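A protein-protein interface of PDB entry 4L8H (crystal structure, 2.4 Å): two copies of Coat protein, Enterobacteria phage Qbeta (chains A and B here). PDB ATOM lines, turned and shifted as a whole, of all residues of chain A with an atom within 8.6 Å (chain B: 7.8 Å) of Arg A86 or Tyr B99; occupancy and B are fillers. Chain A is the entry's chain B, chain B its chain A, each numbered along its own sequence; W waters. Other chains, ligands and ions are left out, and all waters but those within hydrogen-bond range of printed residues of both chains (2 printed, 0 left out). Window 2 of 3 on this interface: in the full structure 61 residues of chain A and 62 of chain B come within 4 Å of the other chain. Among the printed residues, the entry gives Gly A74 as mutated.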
ATOM      1  N   ALA A  43     -21.288 -28.420  -8.504  1.00  0.00           N
ATOM      2  CA  ALA A  43     -20.834 -27.276  -7.690  1.00  0.00           C
ATOM      3  C   ALA A  43     -20.174 -26.180  -8.514  1.00  0.00           C
ATOM      4  O   ALA A  43     -19.929 -25.071  -8.005  1.00  0.00           O
ATOM      5  CB  ALA A  43     -19.859 -27.744  -6.533  1.00  0.00           C
ATOM      6  N   LEU A  44     -19.887 -26.495  -9.770  1.00  0.00           N
ATOM      7  CA  LEU A  44     -19.323 -25.558 -10.717  1.00  0.00           C
ATOM      8  C   LEU A  44     -20.326 -25.022 -11.734  1.00  0.00           C
ATOM      9  O   LEU A  44     -19.945 -24.321 -12.659  1.00  0.00           O
ATOM     10  CB  LEU A  44     -18.212 -26.235 -11.507  1.00  0.00           C
ATOM     11  CG  LEU A  44     -17.024 -26.683 -10.695  1.00  0.00           C
ATOM     12  CD1 LEU A  44     -16.069 -27.401 -11.712  1.00  0.00           C
ATOM     13  CD2 LEU A  44     -16.325 -25.545  -9.935  1.00  0.00           C
ATOM     14  N   GLN A  69     -24.709 -16.655 -10.474  1.00  0.00           N
ATOM     15  CA  GLN A  69     -23.491 -17.037  -9.800  1.00  0.00           C
ATOM     16  C   GLN A  69     -22.687 -17.992 -10.646  1.00  0.00           C
ATOM     17  O   GLN A  69     -23.145 -19.098 -10.952  1.00  0.00           O
ATOM     18  CB  GLN A  69     -23.773 -17.627  -8.426  1.00  0.00           C
ATOM     19  CG  GLN A  69     -22.594 -18.469  -7.900  1.00  0.00           C
ATOM     20  CD  GLN A  69     -22.944 -19.209  -6.606  1.00  0.00           C
ATOM     21  OE1 GLN A  69     -23.927 -18.877  -5.928  1.00  0.00           O
ATOM     22  NE2 GLN A  69     -22.140 -20.208  -6.265  1.00  0.00           N
ATOM     23  N   ASN A  70     -21.492 -17.563 -11.014  1.00  0.00           N
ATOM     24  CA  ASN A  70     -20.634 -18.296 -11.911  1.00  0.00           C
ATOM     25  C   ASN A  70     -19.316 -18.736 -11.231  1.00  0.00           C
ATOM     26  O   ASN A  70     -18.450 -17.918 -10.867  1.00  0.00           O
ATOM     27  CB  ASN A  70     -20.393 -17.491 -13.197  1.00  0.00           C
ATOM     28  CG  ASN A  70     -21.667 -17.272 -13.993  1.00  0.00           C
ATOM     29  OD1 ASN A  70     -22.746 -17.781 -13.636  1.00  0.00           O
ATOM     30  ND2 ASN A  70     -21.564 -16.521 -15.086  1.00  0.00           N
ATOM     31  N   PRO A  71     -19.199 -20.043 -10.981  1.00  0.00           N
ATOM     32  CA  PRO A  71     -17.971 -20.623 -10.410  1.00  0.00           C
ATOM     33  C   PRO A  71     -16.890 -20.835 -11.437  1.00  0.00           C
ATOM     34  O   PRO A  71     -17.170 -21.195 -12.591  1.00  0.00           O
ATOM     35  CB  PRO A  71     -18.426 -21.999  -9.904  1.00  0.00           C
ATOM     36  CG  PRO A  71     -19.932 -21.923  -9.880  1.00  0.00           C
ATOM     37  CD  PRO A  71     -20.325 -20.990 -10.945  1.00  0.00           C
ATOM     38  N   THR A  72     -15.665 -20.589 -11.007  1.00  0.00           N
ATOM     39  CA  THR A  72     -14.498 -21.141 -11.698  1.00  0.00           C
ATOM     40  C   THR A  72     -13.752 -22.152 -10.831  1.00  0.00           C
ATOM     41  O   THR A  72     -13.413 -21.842  -9.698  1.00  0.00           O
ATOM     42  CB  THR A  72     -13.518 -20.040 -12.114  1.00  0.00           C
ATOM     43  OG1 THR A  72     -14.260 -18.992 -12.757  1.00  0.00           O
ATOM     44  CG2 THR A  72     -12.456 -20.616 -13.079  1.00  0.00           C
ATOM     45  N   ALA A  73     -13.515 -23.341 -11.381  1.00  0.00           N
ATOM     46  CA  ALA A  73     -12.627 -24.368 -10.767  1.00  0.00           C
ATOM     47  C   ALA A  73     -11.184 -23.917 -10.447  1.00  0.00           C
ATOM     48  O   ALA A  73     -10.512 -23.249 -11.251  1.00  0.00           O
ATOM     49  CB  ALA A  73     -12.573 -25.593 -11.659  1.00  0.00           C
ATOM     50  N   GLY A  74     -10.704 -24.308  -9.270  1.00  0.00           N
ATOM     51  CA  GLY A  74      -9.308 -24.020  -8.853  1.00  0.00           C
ATOM     52  C   GLY A  74      -8.316 -24.971  -9.515  1.00  0.00           C
ATOM     53  O   GLY A  74      -8.729 -25.970 -10.136  1.00  0.00           O
ATOM     54  N   VAL A  84      -7.504 -22.061  -7.090  1.00  0.00           N
ATOM     55  CA  VAL A  84      -8.434 -21.529  -6.078  1.00  0.00           C
ATOM     56  C   VAL A  84      -9.824 -21.128  -6.641  1.00  0.00           C
ATOM     57  O   VAL A  84      -9.944 -20.134  -7.371  1.00  0.00           O
ATOM     58  CB  VAL A  84      -7.832 -20.310  -5.325  1.00  0.00           C
ATOM     59  CG1 VAL A  84      -8.408 -20.238  -3.868  1.00  0.00           C
ATOM     60  CG2 VAL A  84      -6.265 -20.330  -5.371  1.00  0.00           C
ATOM     61  N   THR A  85     -10.853 -21.916  -6.277  1.00  0.00           N
ATOM     62  CA  THR A  85     -12.253 -21.712  -6.683  1.00  0.00           C
ATOM     63  C   THR A  85     -12.665 -20.238  -6.431  1.00  0.00           C
ATOM     64  O   THR A  85     -12.495 -19.695  -5.330  1.00  0.00           O
ATOM     65  CB  THR A  85     -13.210 -22.747  -5.984  1.00  0.00           C
ATOM     66  OG1 THR A  85     -12.989 -24.052  -6.541  1.00  0.00           O
ATOM     67  CG2 THR A  85     -14.704 -22.409  -6.213  1.00  0.00           C
ATOM     68  N   ARG A  86     -13.136 -19.559  -7.466  1.00  0.00           N
ATOM     69  CA  ARG A  86     -13.685 -18.236  -7.232  1.00  0.00           C
ATOM     70  C   ARG A  86     -15.100 -18.172  -7.802  1.00  0.00           C
ATOM     71  O   ARG A  86     -15.460 -18.955  -8.688  1.00  0.00           O
ATOM     72  CB  ARG A  86     -12.757 -17.125  -7.777  1.00  0.00           C
ATOM     73  CG  ARG A  86     -12.427 -17.222  -9.225  1.00  0.00           C
ATOM     74  CD  ARG A  86     -11.609 -16.027  -9.742  1.00  0.00           C
ATOM     75  NE  ARG A  86     -11.260 -16.277 -11.138  1.00  0.00           N
ATOM     76  CZ  ARG A  86     -10.292 -17.109 -11.525  1.00  0.00           C
ATOM     77  NH1 ARG A  86      -9.516 -17.729 -10.623  1.00  0.00           N
ATOM     78  NH2 ARG A  86     -10.074 -17.295 -12.810  1.00  0.00           N
ATOM     79  N   GLN A  87     -15.882 -17.262  -7.263  1.00  0.00           N
ATOM     80  CA  GLN A  87     -17.246 -17.034  -7.711  1.00  0.00           C
ATOM     81  C   GLN A  87     -17.348 -15.633  -8.298  1.00  0.00           C
ATOM     82  O   GLN A  87     -16.804 -14.695  -7.711  1.00  0.00           O
ATOM     83  CB  GLN A  87     -18.233 -17.133  -6.522  1.00  0.00           C
ATOM     84  CG  GLN A  87     -18.141 -18.416  -5.705  1.00  0.00           C
ATOM     85  CD  GLN A  87     -18.657 -19.602  -6.472  1.00  0.00           C
ATOM     86  OE1 GLN A  87     -19.444 -19.450  -7.401  1.00  0.00           O
ATOM     87  NE2 GLN A  87     -18.215 -20.794  -6.104  1.00  0.00           N
ATOM     88  N   ALA A  88     -18.028 -15.505  -9.447  1.00  0.00           N
ATOM     89  CA  ALA A  88     -18.478 -14.197  -9.923  1.00  0.00           C
ATOM     90  C   ALA A  88     -19.983 -14.074  -9.742  1.00  0.00           C
ATOM     91  O   ALA A  88     -20.734 -14.982 -10.094  1.00  0.00           O
ATOM     92  CB  ALA A  88     -18.127 -14.011 -11.351  1.00  0.00           C
ATOM     93  N   TYR A  89     -20.408 -12.942  -9.206  1.00  0.00           N
ATOM     94  CA  TYR A  89     -21.785 -12.675  -8.876  1.00  0.00           C
ATOM     95  C   TYR A  89     -22.299 -11.434  -9.594  1.00  0.00           C
ATOM     96  O   TYR A  89     -21.564 -10.420  -9.741  1.00  0.00           O
ATOM     97  CB  TYR A  89     -21.943 -12.367  -7.392  1.00  0.00           C
ATOM     98  CG  TYR A  89     -21.488 -13.434  -6.460  1.00  0.00           C
ATOM     99  CD1 TYR A  89     -22.338 -14.499  -6.102  1.00  0.00           C
ATOM    100  CD2 TYR A  89     -20.217 -13.365  -5.863  1.00  0.00           C
ATOM    101  CE1 TYR A  89     -21.915 -15.491  -5.202  1.00  0.00           C
ATOM    102  CE2 TYR A  89     -19.799 -14.332  -4.976  1.00  0.00           C
ATOM    103  CZ  TYR A  89     -20.634 -15.388  -4.650  1.00  0.00           C
ATOM    104  OH  TYR A  89     -20.171 -16.344  -3.759  1.00  0.00           O
ATOM    105  N   LEU A 128     -12.864  -3.205 -15.542  1.00  0.00           N
ATOM    106  CA  LEU A 128     -12.773  -2.612 -14.198  1.00  0.00           C
ATOM    107  C   LEU A 128     -12.234  -1.129 -14.185  1.00  0.00           C
ATOM    108  O   LEU A 128     -11.582  -0.688 -13.237  1.00  0.00           O
ATOM    109  CB  LEU A 128     -11.987  -3.526 -13.236  1.00  0.00           C
ATOM    110  CG  LEU A 128     -12.711  -4.839 -12.822  1.00  0.00           C
ATOM    111  CD1 LEU A 128     -11.748  -5.890 -12.224  1.00  0.00           C
ATOM    112  CD2 LEU A 128     -13.964  -4.654 -11.868  1.00  0.00           C
ATOM    113  N   LYS B  60     -11.858  -7.307   0.070  1.00  0.00           N
ATOM    114  CA  LYS B  60     -10.951  -8.052  -0.817  1.00  0.00           C
ATOM    115  C   LYS B  60     -11.408  -8.151  -2.281  1.00  0.00           C
ATOM    116  O   LYS B  60     -10.649  -8.621  -3.132  1.00  0.00           O
ATOM    117  CB  LYS B  60     -10.669  -9.455  -0.245  1.00  0.00           C
ATOM    118  N   ASN B  61     -12.632  -7.700  -2.584  1.00  0.00           N
ATOM    119  CA  ASN B  61     -13.187  -7.838  -3.947  1.00  0.00           C
ATOM    120  C   ASN B  61     -13.440  -6.527  -4.695  1.00  0.00           C
ATOM    121  O   ASN B  61     -13.567  -5.469  -4.094  1.00  0.00           O
ATOM    122  CB  ASN B  61     -14.472  -8.673  -3.902  1.00  0.00           C
ATOM    123  CG  ASN B  61     -14.275 -10.001  -3.197  1.00  0.00           C
ATOM    124  OD1 ASN B  61     -13.481 -10.848  -3.628  1.00  0.00           O
ATOM    125  ND2 ASN B  61     -14.985 -10.185  -2.093  1.00  0.00           N
ATOM    126  N   TYR B  62     -13.504  -6.617  -6.016  1.00  0.00           N
ATOM    127  CA  TYR B  62     -14.037  -5.545  -6.844  1.00  0.00           C
ATOM    128  C   TYR B  62     -15.570  -5.567  -6.918  1.00  0.00           C
ATOM    129  O   TYR B  62     -16.203  -6.625  -6.867  1.00  0.00           O
ATOM    130  CB  TYR B  62     -13.551  -5.692  -8.253  1.00  0.00           C
ATOM    131  CG  TYR B  62     -12.133  -5.330  -8.492  1.00  0.00           C
ATOM    132  CD1 TYR B  62     -11.784  -4.021  -8.832  1.00  0.00           C
ATOM    133  CD2 TYR B  62     -11.127  -6.305  -8.444  1.00  0.00           C
ATOM    134  CE1 TYR B  62     -10.482  -3.682  -9.113  1.00  0.00           C
ATOM    135  CE2 TYR B  62      -9.804  -5.971  -8.710  1.00  0.00           C
ATOM    136  CZ  TYR B  62      -9.492  -4.662  -9.041  1.00  0.00           C
ATOM    137  OH  TYR B  62      -8.181  -4.317  -9.311  1.00  0.00           O
ATOM    138  N   PHE B  96     -16.627  -9.307  -8.026  1.00  0.00           N
ATOM    139  CA  PHE B  96     -15.558 -10.095  -8.633  1.00  0.00           C
ATOM    140  C   PHE B  96     -14.320 -10.093  -7.724  1.00  0.00           C
ATOM    141  O   PHE B  96     -13.989  -9.104  -7.077  1.00  0.00           O
ATOM    142  CB  PHE B  96     -15.119  -9.543 -10.009  1.00  0.00           C
ATOM    143  CG  PHE B  96     -16.229  -9.354 -11.010  1.00  0.00           C
ATOM    144  CD1 PHE B  96     -16.917 -10.446 -11.540  1.00  0.00           C
ATOM    145  CD2 PHE B  96     -16.555  -8.061 -11.460  1.00  0.00           C
ATOM    146  CE1 PHE B  96     -17.916 -10.267 -12.475  1.00  0.00           C
ATOM    147  CE2 PHE B  96     -17.562  -7.870 -12.431  1.00  0.00           C
ATOM    148  CZ  PHE B  96     -18.250  -8.983 -12.941  1.00  0.00           C
ATOM    149  N   THR B  97     -13.640 -11.218  -7.735  1.00  0.00           N
ATOM    150  CA  THR B  97     -12.363 -11.423  -7.084  1.00  0.00           C
ATOM    151  C   THR B  97     -11.212 -10.735  -7.875  1.00  0.00           C
ATOM    152  O   THR B  97     -11.366 -10.410  -9.075  1.00  0.00           O
ATOM    153  CB  THR B  97     -12.179 -12.980  -7.062  1.00  0.00           C
ATOM    154  OG1 THR B  97     -12.753 -13.530  -5.854  1.00  0.00           O
ATOM    155  CG2 THR B  97     -10.784 -13.396  -7.253  1.00  0.00           C
ATOM    156  N   GLN B  98     -10.053 -10.551  -7.227  1.00  0.00           N
ATOM    157  CA  GLN B  98      -8.860  -9.973  -7.899  1.00  0.00           C
ATOM    158  C   GLN B  98      -8.232 -10.936  -8.909  1.00  0.00           C
ATOM    159  O   GLN B  98      -7.419 -10.512  -9.722  1.00  0.00           O
ATOM    160  CB  GLN B  98      -7.791  -9.588  -6.918  1.00  0.00           C
ATOM    161  CG  GLN B  98      -8.246  -8.763  -5.715  1.00  0.00           C
ATOM    162  CD  GLN B  98      -7.088  -8.521  -4.721  1.00  0.00           C
ATOM    163  OE1 GLN B  98      -6.075  -9.260  -4.726  1.00  0.00           O
ATOM    164  NE2 GLN B  98      -7.234  -7.493  -3.875  1.00  0.00           N
ATOM    165  N   TYR B  99      -8.621 -12.212  -8.870  1.00  0.00           N
ATOM    166  CA  TYR B  99      -8.105 -13.210  -9.812  1.00  0.00           C
ATOM    167  C   TYR B  99      -9.079 -13.513 -10.932  1.00  0.00           C
ATOM    168  O   TYR B  99      -8.835 -14.422 -11.748  1.00  0.00           O
ATOM    169  CB  TYR B  99      -7.741 -14.504  -9.077  1.00  0.00           C
ATOM    170  CG  TYR B  99      -6.757 -14.272  -7.933  1.00  0.00           C
ATOM    171  CD1 TYR B  99      -5.394 -14.036  -8.182  1.00  0.00           C
ATOM    172  CD2 TYR B  99      -7.194 -14.273  -6.602  1.00  0.00           C
ATOM    173  CE1 TYR B  99      -4.496 -13.822  -7.125  1.00  0.00           C
ATOM    174  CE2 TYR B  99      -6.310 -14.066  -5.542  1.00  0.00           C
ATOM    175  CZ  TYR B  99      -4.971 -13.840  -5.808  1.00  0.00           C
ATOM    176  OH  TYR B  99      -4.108 -13.624  -4.748  1.00  0.00           O
ATOM    177  N   SER B 100     -10.199 -12.773 -10.962  1.00  0.00           N
ATOM    178  CA  SER B 100     -11.166 -12.947 -12.030  1.00  0.00           C
ATOM    179  C   SER B 100     -10.499 -12.439 -13.291  1.00  0.00           C
ATOM    180  O   SER B 100      -9.707 -11.496 -13.246  1.00  0.00           O
ATOM    181  CB  SER B 100     -12.451 -12.174 -11.752  1.00  0.00           C
ATOM    182  OG  SER B 100     -12.197 -10.775 -11.656  1.00  0.00           O
ATOM    183  N   THR B 101     -10.823 -13.065 -14.406  1.00  0.00           N
ATOM    184  CA  THR B 101     -10.355 -12.627 -15.689  1.00  0.00           C
ATOM    185  C   THR B 101     -11.434 -11.800 -16.367  1.00  0.00           C
ATOM    186  O   THR B 101     -12.642 -11.894 -16.030  1.00  0.00           O
ATOM    187  CB  THR B 101     -10.126 -13.823 -16.565  1.00  0.00           C
ATOM    188  OG1 THR B 101     -11.394 -14.447 -16.761  1.00  0.00           O
ATOM    189  CG2 THR B 101      -9.123 -14.832 -15.868  1.00  0.00           C
ATOM    190  N   ASP B 102     -11.016 -11.018 -17.370  1.00  0.00           N
ATOM    191  CA  ASP B 102     -11.949 -10.222 -18.132  1.00  0.00           C
ATOM    192  C   ASP B 102     -12.953 -11.110 -18.898  1.00  0.00           C
ATOM    193  O   ASP B 102     -14.115 -10.698 -19.103  1.00  0.00           O
ATOM    194  CB  ASP B 102     -11.195  -9.280 -19.064  1.00  0.00           C
ATOM    195  CG  ASP B 102     -10.419 -10.026 -20.141  1.00  0.00           C
ATOM    196  OD1 ASP B 102      -9.407 -10.758 -19.853  1.00  0.00           O
ATOM    197  OD2 ASP B 102     -10.849  -9.903 -21.291  1.00  0.00           O
ATOM    198  N   GLU B 104     -14.313 -13.804 -17.775  1.00  0.00           N
ATOM    199  CA  GLU B 104     -15.332 -14.152 -16.794  1.00  0.00           C
ATOM    200  C   GLU B 104     -16.280 -12.994 -16.534  1.00  0.00           C
ATOM    201  O   GLU B 104     -17.485 -13.202 -16.391  1.00  0.00           O
ATOM    202  CB  GLU B 104     -14.682 -14.584 -15.468  1.00  0.00           C
ATOM    203  CG  GLU B 104     -14.116 -16.000 -15.534  1.00  0.00           C
ATOM    204  CD  GLU B 104     -13.081 -16.356 -14.419  1.00  0.00           C
ATOM    205  OE1 GLU B 104     -12.816 -15.541 -13.478  1.00  0.00           O
ATOM    206  OE2 GLU B 104     -12.537 -17.503 -14.511  1.00  0.00           O
ATOM    207  N   ARG B 105     -15.739 -11.776 -16.427  1.00  0.00           N
ATOM    208  CA  ARG B 105     -16.571 -10.633 -16.123  1.00  0.00           C
ATOM    209  C   ARG B 105     -17.449 -10.284 -17.321  1.00  0.00           C
ATOM    210  O   ARG B 105     -18.603  -9.996 -17.138  1.00  0.00           O
ATOM    211  CB  ARG B 105     -15.755  -9.429 -15.668  1.00  0.00           C
ATOM    212  CG  ARG B 105     -14.891  -9.705 -14.411  1.00  0.00           C
ATOM    213  CD  ARG B 105     -14.175  -8.414 -13.924  1.00  0.00           C
ATOM    214  NE  ARG B 105     -13.174  -7.993 -14.904  1.00  0.00           N
ATOM    215  CZ  ARG B 105     -11.871  -8.294 -14.870  1.00  0.00           C
ATOM    216  NH1 ARG B 105     -11.346  -8.999 -13.859  1.00  0.00           N
ATOM    217  NH2 ARG B 105     -11.075  -7.828 -15.836  1.00  0.00           N
HETATM  218  O   HOH W   1     -14.785 -13.204  -9.223  1.00  0.00           O
HETATM  219  O   HOH W   2     -18.724 -15.618 -15.613  1.00  0.00           O
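The guanidinium group of Arg A86 sits close to the backbone carbonyl oxygen of Tyr B99 (3.1 Å). OE2 of Glu B104 sits at hydrogen-bond distance from OG1 of Thr A72. The guanidinium group (NE) of Arg A86 lies within salt-bridge range of the side-chain carboxylate (OE1) of Glu B104 (2.9 Å).
The backbone NH (N) of Tyr B62 lies within hydrogen-bond range of the backbone carbonyl oxygen (O) of Phe B96 (2.7 Å). The backbone carbonyl oxygen (O) of Thr B97 lies within hydrogen-bond range of the side-chain hydroxyl (OG) of Ser B100 (2.7 Å). OG of Ser B100 is in hydrogen-bond range of NH1 of Arg B105 (3.0 Å). The backbone NH (N) of Glu B104 lies within hydrogen-bond range of the side-chain hydroxyl (OG1) of Thr B101, 3.2 Å away. O of Asn A70 is in hydrogen-bond range of N of Ala A88 (2.8 Å). The backbone NH (N) of Thr A72 lies within hydrogen-bond range of the backbone carbonyl oxygen (O) of Arg A86 (2.8 Å).
Arg A86 touches Thr B97. NE of Arg A86 touches CA of Ser B100, 3.4 Å away. Ala A88 touches Phe B96. Tyr B62 touches Leu A128 (CB to CD2, 3.8 Å). Leu A128 touches Arg B105.
Of the printed residues of chain B, Arg A86 touches Thr B97, Tyr B99, Ser B100 and Glu B104. Of the printed residues of chain A, Tyr B99 touches Arg A86 (3.1 Å). Ser B100 touches just one residue of chain A: Arg A86 (3.4 Å). Of the printed residues of chain B, Ala A88 touches Phe B96 (3.8 Å). Printed residues of chain B within 4 Å of Leu A128: Tyr B62 and Arg B105. Printed residues of chain A within 4 Å of Phe B96: Ala A88 (3.8 Å). The nearest residue of chain A that does not touch Tyr B99 is Val A84 (6.2 Å).
Hydrophobic or aromatic side chains of chain B within 4 Å of the printed part of chain A: Tyr B62, Phe B96 and Tyr B99. Printed residues of chain A that touch a printed residue of chain B: Thr A72, Arg A86, Ala A88 and Leu A128. Hydrophobic or aromatic side chains of chain A that line the printed part of chain B: Ala A88 and Leu A128. Among the printed residues, 8 pairs touch across the chains.
No position is printed for both chains.
Water W1 bridges N of Thr B97 (2.7 Å) and O of Gln A87 (2.9 Å). Water W2 bridges O of Glu B104 (2.8 Å) and ND2 of Asn A70 (3.0 Å).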
